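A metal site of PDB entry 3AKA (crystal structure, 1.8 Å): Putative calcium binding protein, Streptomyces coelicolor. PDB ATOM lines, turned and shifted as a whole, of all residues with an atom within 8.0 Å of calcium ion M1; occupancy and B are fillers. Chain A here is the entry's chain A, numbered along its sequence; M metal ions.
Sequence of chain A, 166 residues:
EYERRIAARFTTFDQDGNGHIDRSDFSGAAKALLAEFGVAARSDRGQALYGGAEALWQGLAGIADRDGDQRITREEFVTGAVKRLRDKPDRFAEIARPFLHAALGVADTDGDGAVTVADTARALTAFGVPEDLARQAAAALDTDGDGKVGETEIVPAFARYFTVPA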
ATOM      1  N   LEU A 104      -9.783  31.204  -9.878  1.00  0.00           N
ATOM      2  CA  LEU A 104      -9.460  29.991  -9.090  1.00  0.00           C
ATOM      3  C   LEU A 104      -9.077  30.357  -7.646  1.00  0.00           C
ATOM      4  O   LEU A 104      -9.546  29.714  -6.715  1.00  0.00           O
ATOM      5  CB  LEU A 104      -8.349  29.179  -9.749  1.00  0.00           C
ATOM      6  CG  LEU A 104      -8.749  28.401 -11.034  1.00  0.00           C
ATOM      7  CD1 LEU A 104      -7.460  27.850 -11.690  1.00  0.00           C
ATOM      8  CD2 LEU A 104      -9.794  27.275 -10.770  1.00  0.00           C
ATOM      9  N   GLY A 105      -8.246  31.392  -7.483  1.00  0.00           N
ATOM     10  CA  GLY A 105      -7.875  31.901  -6.139  1.00  0.00           C
ATOM     11  C   GLY A 105      -9.084  32.238  -5.280  1.00  0.00           C
ATOM     12  O   GLY A 105      -9.157  31.872  -4.093  1.00  0.00           O
ATOM     13  N   ALA A 107     -12.107  31.122  -5.682  1.00  0.00           N
ATOM     14  CA  ALA A 107     -12.986  29.959  -5.465  1.00  0.00           C
ATOM     15  C   ALA A 107     -12.298  28.870  -4.602  1.00  0.00           C
ATOM     16  O   ALA A 107     -12.899  27.833  -4.279  1.00  0.00           O
ATOM     17  CB  ALA A 107     -13.430  29.404  -6.785  1.00  0.00           C
ATOM     18  N   ASP A 108     -11.039  29.117  -4.270  1.00  0.00           N
ATOM     19  CA  ASP A 108     -10.262  28.242  -3.410  1.00  0.00           C
ATOM     20  C   ASP A 108     -10.478  28.622  -1.918  1.00  0.00           C
ATOM     21  O   ASP A 108      -9.820  29.526  -1.372  1.00  0.00           O
ATOM     22  CB  ASP A 108      -8.787  28.262  -3.822  1.00  0.00           C
ATOM     23  CG  ASP A 108      -7.876  27.535  -2.824  1.00  0.00           C
ATOM     24  OD1 ASP A 108      -8.362  26.660  -2.066  1.00  0.00           O
ATOM     25  OD2 ASP A 108      -6.679  27.896  -2.761  1.00  0.00           O
ATOM     26  N   THR A 109     -11.393  27.912  -1.276  1.00  0.00           N
ATOM     27  CA  THR A 109     -11.886  28.317   0.036  1.00  0.00           C
ATOM     28  C   THR A 109     -11.035  27.859   1.211  1.00  0.00           C
ATOM     29  O   THR A 109     -11.222  28.396   2.299  1.00  0.00           O
ATOM     30  CB  THR A 109     -13.332  27.810   0.277  1.00  0.00           C
ATOM     31  OG1 THR A 109     -13.312  26.381   0.324  1.00  0.00           O
ATOM     32  CG2 THR A 109     -14.257  28.294  -0.837  1.00  0.00           C
ATOM     33  N   ASP A 110     -10.167  26.858   1.014  1.00  0.00           N
ATOM     34  CA  ASP A 110      -9.255  26.442   2.089  1.00  0.00           C
ATOM     35  C   ASP A 110      -7.810  26.859   1.843  1.00  0.00           C
ATOM     36  O   ASP A 110      -6.943  26.627   2.672  1.00  0.00           O
ATOM     37  CB  ASP A 110      -9.385  24.951   2.422  1.00  0.00           C
ATOM     38  CG  ASP A 110      -8.975  24.043   1.259  1.00  0.00           C
ATOM     39  OD1 ASP A 110      -8.566  24.545   0.200  1.00  0.00           O
ATOM     40  OD2 ASP A 110      -9.054  22.793   1.402  1.00  0.00           O
ATOM     41  N   GLY A 111      -7.552  27.483   0.688  1.00  0.00           N
ATOM     42  CA  GLY A 111      -6.223  28.019   0.400  1.00  0.00           C
ATOM     43  C   GLY A 111      -5.147  27.037  -0.046  1.00  0.00           C
ATOM     44  O   GLY A 111      -3.961  27.392  -0.118  1.00  0.00           O
ATOM     45  N   ASP A 112      -5.544  25.803  -0.378  1.00  0.00           N
ATOM     46  CA  ASP A 112      -4.596  24.740  -0.785  1.00  0.00           C
ATOM     47  C   ASP A 112      -4.280  24.774  -2.264  1.00  0.00           C
ATOM     48  O   ASP A 112      -3.610  23.871  -2.796  1.00  0.00           O
ATOM     49  CB  ASP A 112      -5.106  23.335  -0.371  1.00  0.00           C
ATOM     50  CG  ASP A 112      -6.346  22.917  -1.106  1.00  0.00           C
ATOM     51  OD1 ASP A 112      -6.727  23.568  -2.116  1.00  0.00           O
ATOM     52  OD2 ASP A 112      -6.989  21.938  -0.674  1.00  0.00           O
ATOM     53  N   GLY A 113      -4.795  25.800  -2.954  1.00  0.00           N
ATOM     54  CA  GLY A 113      -4.473  25.991  -4.349  1.00  0.00           C
ATOM     55  C   GLY A 113      -5.284  25.157  -5.316  1.00  0.00           C
ATOM     56  O   GLY A 113      -4.972  25.112  -6.515  1.00  0.00           O
ATOM     57  N   ALA A 114      -6.334  24.503  -4.802  1.00  0.00           N
ATOM     58  CA  ALA A 114      -7.195  23.653  -5.616  1.00  0.00           C
ATOM     59  C   ALA A 114      -8.633  24.113  -5.400  1.00  0.00           C
ATOM     60  O   ALA A 114      -8.932  24.708  -4.393  1.00  0.00           O
ATOM     61  CB  ALA A 114      -7.034  22.187  -5.169  1.00  0.00           C
ATOM     62  N   VAL A 115      -9.520  23.874  -6.369  1.00  0.00           N
ATOM     63  CA  VAL A 115     -10.934  24.264  -6.253  1.00  0.00           C
ATOM     64  C   VAL A 115     -11.807  23.000  -6.383  1.00  0.00           C
ATOM     65  O   VAL A 115     -11.533  22.161  -7.257  1.00  0.00           O
ATOM     66  CB  VAL A 115     -11.325  25.269  -7.382  1.00  0.00           C
ATOM     67  CG1 VAL A 115     -12.820  25.616  -7.366  1.00  0.00           C
ATOM     68  CG2 VAL A 115     -10.528  26.552  -7.259  1.00  0.00           C
ATOM     69  N   THR A 116     -12.844  22.860  -5.547  1.00  0.00           N
ATOM     70  CA  THR A 116     -13.718  21.665  -5.627  1.00  0.00           C
ATOM     71  C   THR A 116     -14.649  21.814  -6.834  1.00  0.00           C
ATOM     72  O   THR A 116     -14.845  22.927  -7.367  1.00  0.00           O
ATOM     73  CB  THR A 116     -14.575  21.506  -4.344  1.00  0.00           C
ATOM     74  OG1 THR A 116     -15.479  22.603  -4.248  1.00  0.00           O
ATOM     75  CG2 THR A 116     -13.695  21.470  -3.109  1.00  0.00           C
ATOM     76  N   ASP A 119     -17.523  24.125  -5.873  1.00  0.00           N
ATOM     77  CA  ASP A 119     -17.167  25.530  -5.923  1.00  0.00           C
ATOM     78  C   ASP A 119     -16.916  26.045  -7.355  1.00  0.00           C
ATOM     79  O   ASP A 119     -17.119  27.246  -7.655  1.00  0.00           O
ATOM     80  CB  ASP A 119     -15.981  25.806  -4.999  1.00  0.00           C
ATOM     81  CG  ASP A 119     -16.360  25.672  -3.525  1.00  0.00           C
ATOM     82  OD1 ASP A 119     -17.553  25.833  -3.190  1.00  0.00           O
ATOM     83  OD2 ASP A 119     -15.442  25.453  -2.703  1.00  0.00           O
ATOM     84  N   LYS A 148     -11.057  17.791  -8.088  1.00  0.00           N
ATOM     85  CA  LYS A 148     -10.389  19.087  -7.974  1.00  0.00           C
ATOM     86  C   LYS A 148     -10.293  19.664  -9.364  1.00  0.00           C
ATOM     87  O   LYS A 148      -9.937  18.957 -10.325  1.00  0.00           O
ATOM     88  CB  LYS A 148      -9.018  18.943  -7.348  1.00  0.00           C
ATOM     89  CG  LYS A 148      -9.052  18.212  -5.998  1.00  0.00           C
ATOM     90  CD  LYS A 148      -7.693  18.158  -5.362  1.00  0.00           C
ATOM     91  CE  LYS A 148      -7.738  17.328  -4.102  1.00  0.00           C
ATOM     92  NZ  LYS A 148      -7.522  15.888  -4.477  1.00  0.00           N
ATOM     93  N   VAL A 149     -10.643  20.948  -9.497  1.00  0.00           N
ATOM     94  CA  VAL A 149     -10.610  21.606 -10.787  1.00  0.00           C
ATOM     95  C   VAL A 149      -9.477  22.631 -10.778  1.00  0.00           C
ATOM     96  O   VAL A 149      -9.362  23.439  -9.849  1.00  0.00           O
ATOM     97  CB  VAL A 149     -12.004  22.243 -11.084  1.00  0.00           C
ATOM     98  CG1 VAL A 149     -11.978  23.150 -12.331  1.00  0.00           C
ATOM     99  CG2 VAL A 149     -13.038  21.137 -11.249  1.00  0.00           C
HETATM  100 CA    CA M   1      -8.957  24.514  -2.018  1.00  0.00          CA
HETATM  101 CA    CA M   2     -11.202  24.969  -1.600  1.00  0.00          CA
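Calcium ion M1 is bound by the side-chain carboxylate (OD1) of Asp 108 (2.2 Å).
Calcium ion M1 is bound by the side-chain carboxylate (OD1) of Asp 110 (2.3 Å).
O of Ala 114 binds calcium ion M1.
OD1 of Asp 112 is bound to calcium ion M1 (2.4 Å).
Calcium ion M1 has four donor atoms within binding distance.
The backbone NH of Gly 113 lies within hydrogen-bond range of the side-chain carboxylate of Asp 108.
N of Gly 111 sits close to OD1 of Asp 108 (3.0 Å).
The nearest printed residue that does not touch calcium ion M1 is Thr 109 (4.2 Å).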
